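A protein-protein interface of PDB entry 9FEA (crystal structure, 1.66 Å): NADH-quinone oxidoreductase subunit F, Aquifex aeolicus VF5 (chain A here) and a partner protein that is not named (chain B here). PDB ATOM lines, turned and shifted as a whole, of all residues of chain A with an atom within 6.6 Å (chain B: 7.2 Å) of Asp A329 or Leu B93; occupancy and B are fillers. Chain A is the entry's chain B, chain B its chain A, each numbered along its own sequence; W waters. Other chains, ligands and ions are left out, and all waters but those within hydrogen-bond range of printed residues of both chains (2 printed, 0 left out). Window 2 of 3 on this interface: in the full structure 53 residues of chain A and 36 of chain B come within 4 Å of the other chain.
Among the printed residues, pairs that only touch across the chains: Gly A256 with Val B90 (3.7 Å), Gly A256 with Met B94 (3.95 Å), Lys A257 with Met B94 (3.8 Å), Ile A323 with Val B90 (3.7 Å), Asp A329 with Leu B93 (3.8 Å), Ala A334 with Ile B89 (3.6 Å), Lys A337 with Ile B89 (3.9 Å) and Lys A337 with His B92 (3.4 Å).
OE2 of Glu A333 is in hydrogen-bond range of NE2 of His B92, at 2.6 Å.
Of chain B, only Leu B93 (3.8 Å) comes within 4 Å of Asp A329. Leu B93 touches one residue of chain A. Printed residues of chain A within 4 Å of Val B90: Gly A256 and Ile A323. Printed residues of chain B within 4 Å of Gly A256: Val B90 and Met B94. The nearest residue of chain B that does not touch Asp A329 is Met B94 (6.9 Å).
Water W1 lies within hydrogen-bond range of O of Leu B93 (2.7 Å), NZ of Lys A257 (3.1 Å) and OD1 of Asp A329 (3.2 Å). Water W2 lies within hydrogen-bond range of N of Ile B89 (3.0 Å) and O of Lys A337 (3.0 Å).
The backbone NH (N) of His B92 lies within hydrogen-bond range of the side-chain hydroxyl (OG1) of Thr B96 (3.3 Å). N of Lys A257 lies within hydrogen-bond range of O of Val A324. The side-chain amino group (NZ) of Lys A257 is in salt-bridge range of the side-chain carboxylate (OD1) of Asp A329, 2.8 Å away. NZ of Lys A290 sits at hydrogen-bond distance from O of Asp A329, 2.7 Å away. The backbone NH (N) of Thr A326 sits at hydrogen-bond distance from the side-chain carboxylate (OD2) of Asp A329 (2.9 Å). The side-chain carboxylate (OD1) of Asp A330 sits at hydrogen-bond distance from the backbone NH (N) of Glu A333.
Of the 18 printed residues of chain A, 7 touch a printed residue of chain B. Printed residues of chain A that touch a printed residue of chain B: Gly A256, Lys A257, Ile A323, Asp A329, Glu A333, Ala A334 and Lys A337. Hydrophobic or aromatic side chains of chain A that line the printed part of chain B: Ile A323 and Ala A334. Of the 10 printed residues of chain B, 5 touch a printed residue of chain A. Hydrophobic or aromatic side chains of chain B that line the printed part of chain A: Ile B89, Val B90, His B92, Leu B93 and Met B94. Among the printed residues, 9 pairs touch across the chains. Among the printed residues, no Asp or Glu carboxylate lies within 4 Å of a Lys or Arg side-chain nitrogen of the other chain.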
ATOM      1  N   GLY A 256     -23.451  -2.082  11.134  1.00  0.00           N
ATOM      2  CA  GLY A 256     -22.395  -2.941  10.654  1.00  0.00           C
ATOM      3  C   GLY A 256     -21.136  -2.122  10.382  1.00  0.00           C
ATOM      4  O   GLY A 256     -20.773  -1.220  11.142  1.00  0.00           O
ATOM      5  N   LYS A 257     -20.475  -2.461   9.280  1.00  0.00           N
ATOM      6  CA  LYS A 257     -19.095  -2.086   9.065  1.00  0.00           C
ATOM      7  C   LYS A 257     -19.007  -0.728   8.376  1.00  0.00           C
ATOM      8  O   LYS A 257     -18.275  -0.590   7.393  1.00  0.00           O
ATOM      9  CB  LYS A 257     -18.418  -3.190   8.243  1.00  0.00           C
ATOM     10  CG  LYS A 257     -18.417  -4.531   8.945  1.00  0.00           C
ATOM     11  CD  LYS A 257     -17.532  -4.516  10.182  1.00  0.00           C
ATOM     12  CE  LYS A 257     -17.405  -5.854  10.839  1.00  0.00           C
ATOM     13  NZ  LYS A 257     -16.592  -6.831  10.108  1.00  0.00           N
ATOM     14  N   LYS A 287     -12.375  -1.038   4.033  1.00  0.00           N
ATOM     15  CA  LYS A 287     -12.442  -2.354   3.431  1.00  0.00           C
ATOM     16  C   LYS A 287     -13.551  -2.354   2.381  1.00  0.00           C
ATOM     17  O   LYS A 287     -14.466  -1.534   2.442  1.00  0.00           O
ATOM     18  CB  LYS A 287     -12.684  -3.381   4.535  1.00  0.00           C
ATOM     19  CG  LYS A 287     -11.514  -3.630   5.475  1.00  0.00           C
ATOM     20  CD  LYS A 287     -12.006  -4.499   6.632  1.00  0.00           C
ATOM     21  CE  LYS A 287     -11.012  -5.387   7.322  1.00  0.00           C
ATOM     22  NZ  LYS A 287     -11.770  -6.345   8.149  1.00  0.00           N
ATOM     23  N   LYS A 290     -18.838  -6.208   0.892  1.00  0.00           N
ATOM     24  CA  LYS A 290     -19.111  -7.546   0.389  1.00  0.00           C
ATOM     25  C   LYS A 290     -20.613  -7.714   0.164  1.00  0.00           C
ATOM     26  O   LYS A 290     -21.058  -8.207  -0.866  1.00  0.00           O
ATOM     27  CB  LYS A 290     -18.623  -8.616   1.369  1.00  0.00           C
ATOM     28  CG  LYS A 290     -19.039 -10.029   0.972  1.00  0.00           C
ATOM     29  CD  LYS A 290     -18.569 -11.102   1.944  1.00  0.00           C
ATOM     30  CE  LYS A 290     -17.151 -11.451   1.763  1.00  0.00           C
ATOM     31  NZ  LYS A 290     -16.878 -12.692   2.498  1.00  0.00           N
ATOM     32  N   ILE A 323     -27.514  -3.045   6.739  1.00  0.00           N
ATOM     33  CA  ILE A 323     -26.456  -3.706   7.485  1.00  0.00           C
ATOM     34  C   ILE A 323     -25.311  -3.995   6.531  1.00  0.00           C
ATOM     35  O   ILE A 323     -25.480  -4.767   5.602  1.00  0.00           O
ATOM     36  CB  ILE A 323     -26.958  -5.023   8.100  1.00  0.00           C
ATOM     37  CG1 ILE A 323     -28.169  -4.837   8.980  1.00  0.00           C
ATOM     38  CG2 ILE A 323     -25.811  -5.698   8.845  1.00  0.00           C
ATOM     39  CD1 ILE A 323     -28.866  -6.134   9.362  1.00  0.00           C
ATOM     40  N   VAL A 324     -24.131  -3.418   6.779  1.00  0.00           N
ATOM     41  CA  VAL A 324     -23.020  -3.533   5.851  1.00  0.00           C
ATOM     42  C   VAL A 324     -22.034  -4.608   6.329  1.00  0.00           C
ATOM     43  O   VAL A 324     -21.555  -4.562   7.466  1.00  0.00           O
ATOM     44  CB  VAL A 324     -22.328  -2.163   5.682  1.00  0.00           C
ATOM     45  CG1 VAL A 324     -21.127  -2.285   4.764  1.00  0.00           C
ATOM     46  CG2 VAL A 324     -23.293  -1.079   5.197  1.00  0.00           C
ATOM     47  N   LEU A 325     -21.747  -5.565   5.435  1.00  0.00           N
ATOM     48  CA  LEU A 325     -20.690  -6.552   5.622  1.00  0.00           C
ATOM     49  C   LEU A 325     -19.539  -6.233   4.675  1.00  0.00           C
ATOM     50  O   LEU A 325     -19.769  -5.865   3.526  1.00  0.00           O
ATOM     51  CB  LEU A 325     -21.200  -7.966   5.351  1.00  0.00           C
ATOM     52  CG  LEU A 325     -22.168  -8.545   6.386  1.00  0.00           C
ATOM     53  CD1 LEU A 325     -23.511  -7.896   6.369  1.00  0.00           C
ATOM     54  CD2 LEU A 325     -22.311 -10.038   6.107  1.00  0.00           C
ATOM     55  N   THR A 326     -18.299  -6.335   5.165  1.00  0.00           N
ATOM     56  CA  THR A 326     -17.141  -6.065   4.325  1.00  0.00           C
ATOM     57  C   THR A 326     -16.427  -7.369   3.998  1.00  0.00           C
ATOM     58  O   THR A 326     -16.875  -8.445   4.385  1.00  0.00           O
ATOM     59  CB  THR A 326     -16.217  -5.026   4.970  1.00  0.00           C
ATOM     60  OG1 THR A 326     -15.957  -5.428   6.307  1.00  0.00           O
ATOM     61  CG2 THR A 326     -16.831  -3.639   4.962  1.00  0.00           C
ATOM     62  N   GLU A 327     -15.306  -7.239   3.276  1.00  0.00           N
ATOM     63  CA  GLU A 327     -14.671  -8.335   2.554  1.00  0.00           C
ATOM     64  C   GLU A 327     -14.234  -9.490   3.453  1.00  0.00           C
ATOM     65  O   GLU A 327     -14.165 -10.622   2.981  1.00  0.00           O
ATOM     66  CB  GLU A 327     -13.456  -7.837   1.771  1.00  0.00           C
ATOM     67  CG  GLU A 327     -12.493  -6.986   2.593  1.00  0.00           C
ATOM     68  CD  GLU A 327     -11.335  -6.441   1.783  1.00  0.00           C
ATOM     69  OE1 GLU A 327     -10.483  -7.268   1.391  1.00  0.00           O
ATOM     70  OE2 GLU A 327     -11.301  -5.226   1.507  1.00  0.00           O
ATOM     71  N   GLU A 328     -13.933  -9.233   4.729  1.00  0.00           N
ATOM     72  CA  GLU A 328     -13.489 -10.314   5.596  1.00  0.00           C
ATOM     73  C   GLU A 328     -14.648 -11.005   6.318  1.00  0.00           C
ATOM     74  O   GLU A 328     -14.405 -12.004   6.990  1.00  0.00           O
ATOM     75  CB  GLU A 328     -12.437  -9.849   6.597  1.00  0.00           C
ATOM     76  CG  GLU A 328     -11.140  -9.442   5.901  1.00  0.00           C
ATOM     77  CD  GLU A 328      -9.952  -9.335   6.832  1.00  0.00           C
ATOM     78  OE1 GLU A 328      -9.534 -10.382   7.381  1.00  0.00           O
ATOM     79  OE2 GLU A 328      -9.455  -8.203   6.988  1.00  0.00           O
ATOM     80  N   ASP A 329     -15.889 -10.544   6.148  1.00  0.00           N
ATOM     81  CA  ASP A 329     -17.013 -11.154   6.853  1.00  0.00           C
ATOM     82  C   ASP A 329     -17.471 -12.439   6.160  1.00  0.00           C
ATOM     83  O   ASP A 329     -17.861 -12.424   4.996  1.00  0.00           O
ATOM     84  CB  ASP A 329     -18.140 -10.159   7.060  1.00  0.00           C
ATOM     85  CG  ASP A 329     -17.763  -9.014   7.987  1.00  0.00           C
ATOM     86  OD1 ASP A 329     -17.116  -9.327   9.021  1.00  0.00           O
ATOM     87  OD2 ASP A 329     -18.096  -7.832   7.666  1.00  0.00           O
ATOM     88  N   ASP A 330     -17.526 -13.534   6.932  1.00  0.00           N
ATOM     89  CA  ASP A 330     -17.899 -14.840   6.406  1.00  0.00           C
ATOM     90  C   ASP A 330     -19.403 -14.840   6.096  1.00  0.00           C
ATOM     91  O   ASP A 330     -20.210 -14.654   6.995  1.00  0.00           O
ATOM     92  CB  ASP A 330     -17.470 -15.912   7.399  1.00  0.00           C
ATOM     93  CG  ASP A 330     -17.742 -17.355   6.998  1.00  0.00           C
ATOM     94  OD1 ASP A 330     -18.822 -17.613   6.464  1.00  0.00           O
ATOM     95  OD2 ASP A 330     -16.852 -18.199   7.203  1.00  0.00           O
ATOM     96  N   ILE A 331     -19.786 -15.078   4.835  1.00  0.00           N
ATOM     97  CA  ILE A 331     -21.186 -14.985   4.450  1.00  0.00           C
ATOM     98  C   ILE A 331     -22.005 -16.127   5.054  1.00  0.00           C
ATOM     99  O   ILE A 331     -23.201 -15.949   5.302  1.00  0.00           O
ATOM    100  CB  ILE A 331     -21.385 -14.900   2.925  1.00  0.00           C
ATOM    101  CG1 ILE A 331     -22.727 -14.247   2.575  1.00  0.00           C
ATOM    102  CG2 ILE A 331     -21.227 -16.264   2.260  1.00  0.00           C
ATOM    103  CD1 ILE A 331     -22.816 -12.774   2.955  1.00  0.00           C
ATOM    104  N   VAL A 332     -21.387 -17.284   5.261  1.00  0.00           N
ATOM    105  CA  VAL A 332     -22.086 -18.438   5.804  1.00  0.00           C
ATOM    106  C   VAL A 332     -22.372 -18.216   7.289  1.00  0.00           C
ATOM    107  O   VAL A 332     -23.456 -18.555   7.765  1.00  0.00           O
ATOM    108  CB  VAL A 332     -21.318 -19.743   5.542  1.00  0.00           C
ATOM    109  CG1 VAL A 332     -22.006 -20.945   6.182  1.00  0.00           C
ATOM    110  CG2 VAL A 332     -21.129 -19.963   4.052  1.00  0.00           C
ATOM    111  N   GLU A 333     -21.406 -17.628   8.005  1.00  0.00           N
ATOM    112  CA  GLU A 333     -21.583 -17.291   9.409  1.00  0.00           C
ATOM    113  C   GLU A 333     -22.710 -16.270   9.558  1.00  0.00           C
ATOM    114  O   GLU A 333     -23.554 -16.365  10.458  1.00  0.00           O
ATOM    115  CB  GLU A 333     -20.249 -16.742   9.920  1.00  0.00           C
ATOM    116  CG  GLU A 333     -20.220 -16.365  11.396  1.00  0.00           C
ATOM    117  CD  GLU A 333     -18.889 -15.708  11.777  1.00  0.00           C
ATOM    118  OE1 GLU A 333     -17.941 -15.679  10.948  1.00  0.00           O
ATOM    119  OE2 GLU A 333     -18.788 -15.203  12.909  1.00  0.00           O
ATOM    120  N   ALA A 334     -22.753 -15.293   8.651  1.00  0.00           N
ATOM    121  CA  ALA A 334     -23.812 -14.299   8.695  1.00  0.00           C
ATOM    122  C   ALA A 334     -25.166 -14.940   8.394  1.00  0.00           C
ATOM    123  O   ALA A 334     -26.162 -14.646   9.046  1.00  0.00           O
ATOM    124  CB  ALA A 334     -23.479 -13.162   7.751  1.00  0.00           C
ATOM    125  N   LYS A 337     -26.666 -16.626  11.361  1.00  0.00           N
ATOM    126  CA  LYS A 337     -27.314 -15.687  12.277  1.00  0.00           C
ATOM    127  C   LYS A 337     -28.733 -15.354  11.803  1.00  0.00           C
ATOM    128  O   LYS A 337     -29.647 -15.248  12.617  1.00  0.00           O
ATOM    129  CB  LYS A 337     -26.460 -14.432  12.492  1.00  0.00           C
ATOM    130  CG  LYS A 337     -25.202 -14.683  13.311  1.00  0.00           C
ATOM    131  CD  LYS A 337     -25.537 -14.907  14.784  1.00  0.00           C
ATOM    132  CE  LYS A 337     -24.457 -15.552  15.548  1.00  0.00           C
ATOM    133  NZ  LYS A 337     -24.476 -17.010  15.467  1.00  0.00           N
ATOM    134  N   GLU A 413     -18.088 -19.110  -1.722  1.00  0.00           N
ATOM    135  CA  GLU A 413     -17.916 -19.190  -0.277  1.00  0.00           C
ATOM    136  C   GLU A 413     -18.646 -20.393   0.315  1.00  0.00           C
ATOM    137  O   GLU A 413     -18.125 -21.053   1.207  1.00  0.00           O
ATOM    138  CB  GLU A 413     -18.446 -17.995   0.508  1.00  0.00           C
ATOM    139  CG  GLU A 413     -17.402 -16.912   0.731  1.00  0.00           C
ATOM    140  CD  GLU A 413     -17.916 -15.755   1.572  1.00  0.00           C
ATOM    141  OE1 GLU A 413     -18.085 -14.692   0.977  1.00  0.00           O
ATOM    142  OE2 GLU A 413     -18.102 -15.886   2.787  1.00  0.00           O
ATOM    143  N   SER B  88     -27.903 -11.519  17.791  1.00  0.00           N
ATOM    144  CA  SER B  88     -28.293 -11.446  16.390  1.00  0.00           C
ATOM    145  C   SER B  88     -27.163 -10.883  15.528  1.00  0.00           C
ATOM    146  O   SER B  88     -26.067 -10.565  16.006  1.00  0.00           O
ATOM    147  CB  SER B  88     -29.544 -10.615  16.225  1.00  0.00           C
ATOM    148  OG  SER B  88     -30.644 -11.255  16.822  1.00  0.00           O
ATOM    149  N   ILE B  89     -27.441 -10.814  14.225  1.00  0.00           N
ATOM    150  CA  ILE B  89     -26.428 -10.617  13.199  1.00  0.00           C
ATOM    151  C   ILE B  89     -25.499  -9.438  13.485  1.00  0.00           C
ATOM    152  O   ILE B  89     -24.274  -9.607  13.385  1.00  0.00           O
ATOM    153  CB  ILE B  89     -27.059 -10.525  11.800  1.00  0.00           C
ATOM    154  CG1 ILE B  89     -26.013 -10.206  10.722  1.00  0.00           C
ATOM    155  CG2 ILE B  89     -28.200  -9.512  11.758  1.00  0.00           C
ATOM    156  CD1 ILE B  89     -25.081 -11.340  10.423  1.00  0.00           C
ATOM    157  N   VAL B  90     -26.039  -8.235  13.730  1.00  0.00           N
ATOM    158  CA  VAL B  90     -25.184  -7.052  13.778  1.00  0.00           C
ATOM    159  C   VAL B  90     -24.270  -7.106  14.999  1.00  0.00           C
ATOM    160  O   VAL B  90     -23.056  -6.910  14.889  1.00  0.00           O
ATOM    161  CB  VAL B  90     -25.906  -5.699  13.663  1.00  0.00           C
ATOM    162  CG1 VAL B  90     -24.925  -4.552  13.458  1.00  0.00           C
ATOM    163  CG2 VAL B  90     -26.883  -5.722  12.513  1.00  0.00           C
ATOM    164  N   CYS B  91     -24.828  -7.440  16.155  1.00  0.00           N
ATOM    165  CA  CYS B  91     -24.009  -7.544  17.350  1.00  0.00           C
ATOM    166  C   CYS B  91     -22.972  -8.656  17.196  1.00  0.00           C
ATOM    167  O   CYS B  91     -21.843  -8.503  17.645  1.00  0.00           O
ATOM    168  CB  CYS B  91     -24.883  -7.674  18.587  1.00  0.00           C
ATOM    169  SG  CYS B  91     -25.843  -6.164  18.894  1.00  0.00           S
ATOM    170  N   HIS B  92     -23.328  -9.724  16.484  1.00  0.00           N
ATOM    171  CA  HIS B  92     -22.398 -10.807  16.257  1.00  0.00           C
ATOM    172  C   HIS B  92     -21.188 -10.303  15.475  1.00  0.00           C
ATOM    173  O   HIS B  92     -20.054 -10.585  15.863  1.00  0.00           O
ATOM    174  CB  HIS B  92     -23.062 -11.998  15.568  1.00  0.00           C
ATOM    175  CG  HIS B  92     -22.062 -13.093  15.383  1.00  0.00           C
ATOM    176  ND1 HIS B  92     -21.631 -13.914  16.407  1.00  0.00           N
ATOM    177  CD2 HIS B  92     -21.385 -13.447  14.294  1.00  0.00           C
ATOM    178  CE1 HIS B  92     -20.721 -14.749  15.934  1.00  0.00           C
ATOM    179  NE2 HIS B  92     -20.557 -14.482  14.643  1.00  0.00           N
ATOM    180  N   LEU B  93     -21.454  -9.601  14.364  1.00  0.00           N
ATOM    181  CA  LEU B  93     -20.425  -8.978  13.541  1.00  0.00           C
ATOM    182  C   LEU B  93     -19.505  -8.092  14.366  1.00  0.00           C
ATOM    183  O   LEU B  93     -18.303  -8.073  14.102  1.00  0.00           O
ATOM    184  CB  LEU B  93     -21.027  -8.110  12.440  1.00  0.00           C
ATOM    185  CG  LEU B  93     -21.672  -8.844  11.272  1.00  0.00           C
ATOM    186  CD1 LEU B  93     -22.370  -7.826  10.384  1.00  0.00           C
ATOM    187  CD2 LEU B  93     -20.610  -9.627  10.526  1.00  0.00           C
ATOM    188  N   MET B  94     -20.085  -7.321  15.285  1.00  0.00           N
ATOM    189  CA  MET B  94     -19.385  -6.226  15.930  1.00  0.00           C
ATOM    190  C   MET B  94     -18.854  -6.590  17.314  1.00  0.00           C
ATOM    191  O   MET B  94     -18.197  -5.743  17.925  1.00  0.00           O
ATOM    192  CB  MET B  94     -20.274  -4.981  16.053  1.00  0.00           C
ATOM    193  CG  MET B  94     -20.849  -4.522  14.727  1.00  0.00           C
ATOM    194  SD  MET B  94     -19.622  -4.266  13.431  1.00  0.00           S
ATOM    195  CE  MET B  94     -18.869  -2.831  14.210  1.00  0.00           C
ATOM    196  N   GLY B  95     -19.126  -7.799  17.824  1.00  0.00           N
ATOM    197  CA  GLY B  95     -18.368  -8.294  18.967  1.00  0.00           C
ATOM    198  C   GLY B  95     -19.175  -8.922  20.109  1.00  0.00           C
ATOM    199  O   GLY B  95     -18.693  -8.927  21.236  1.00  0.00           O
ATOM    200  N   THR B  96     -20.347  -9.522  19.845  1.00  0.00           N
ATOM    201  CA  THR B  96     -21.058 -10.238  20.897  1.00  0.00           C
ATOM    202  C   THR B  96     -20.086 -11.122  21.683  1.00  0.00           C
ATOM    203  O   THR B  96     -20.159 -11.184  22.898  1.00  0.00           O
ATOM    204  CB  THR B  96     -22.202 -11.086  20.336  1.00  0.00           C
ATOM    205  OG1 THR B  96     -23.118 -10.171  19.747  1.00  0.00           O
ATOM    206  CG2 THR B  96     -22.918 -11.881  21.411  1.00  0.00           C
ATOM    207  N   ALA B 134     -23.928  -1.640  18.339  1.00  0.00           N
ATOM    208  CA  ALA B 134     -23.475  -3.011  18.561  1.00  0.00           C
ATOM    209  C   ALA B 134     -22.061  -3.076  19.131  1.00  0.00           C
ATOM    210  O   ALA B 134     -21.201  -2.261  18.765  1.00  0.00           O
ATOM    211  CB  ALA B 134     -23.521  -3.779  17.255  1.00  0.00           C
HETATM  212  O   HOH W   1     -16.689  -9.118  12.160  1.00  0.00           O
HETATM  213  O   HOH W   2     -29.843 -12.380  13.511  1.00  0.00           O
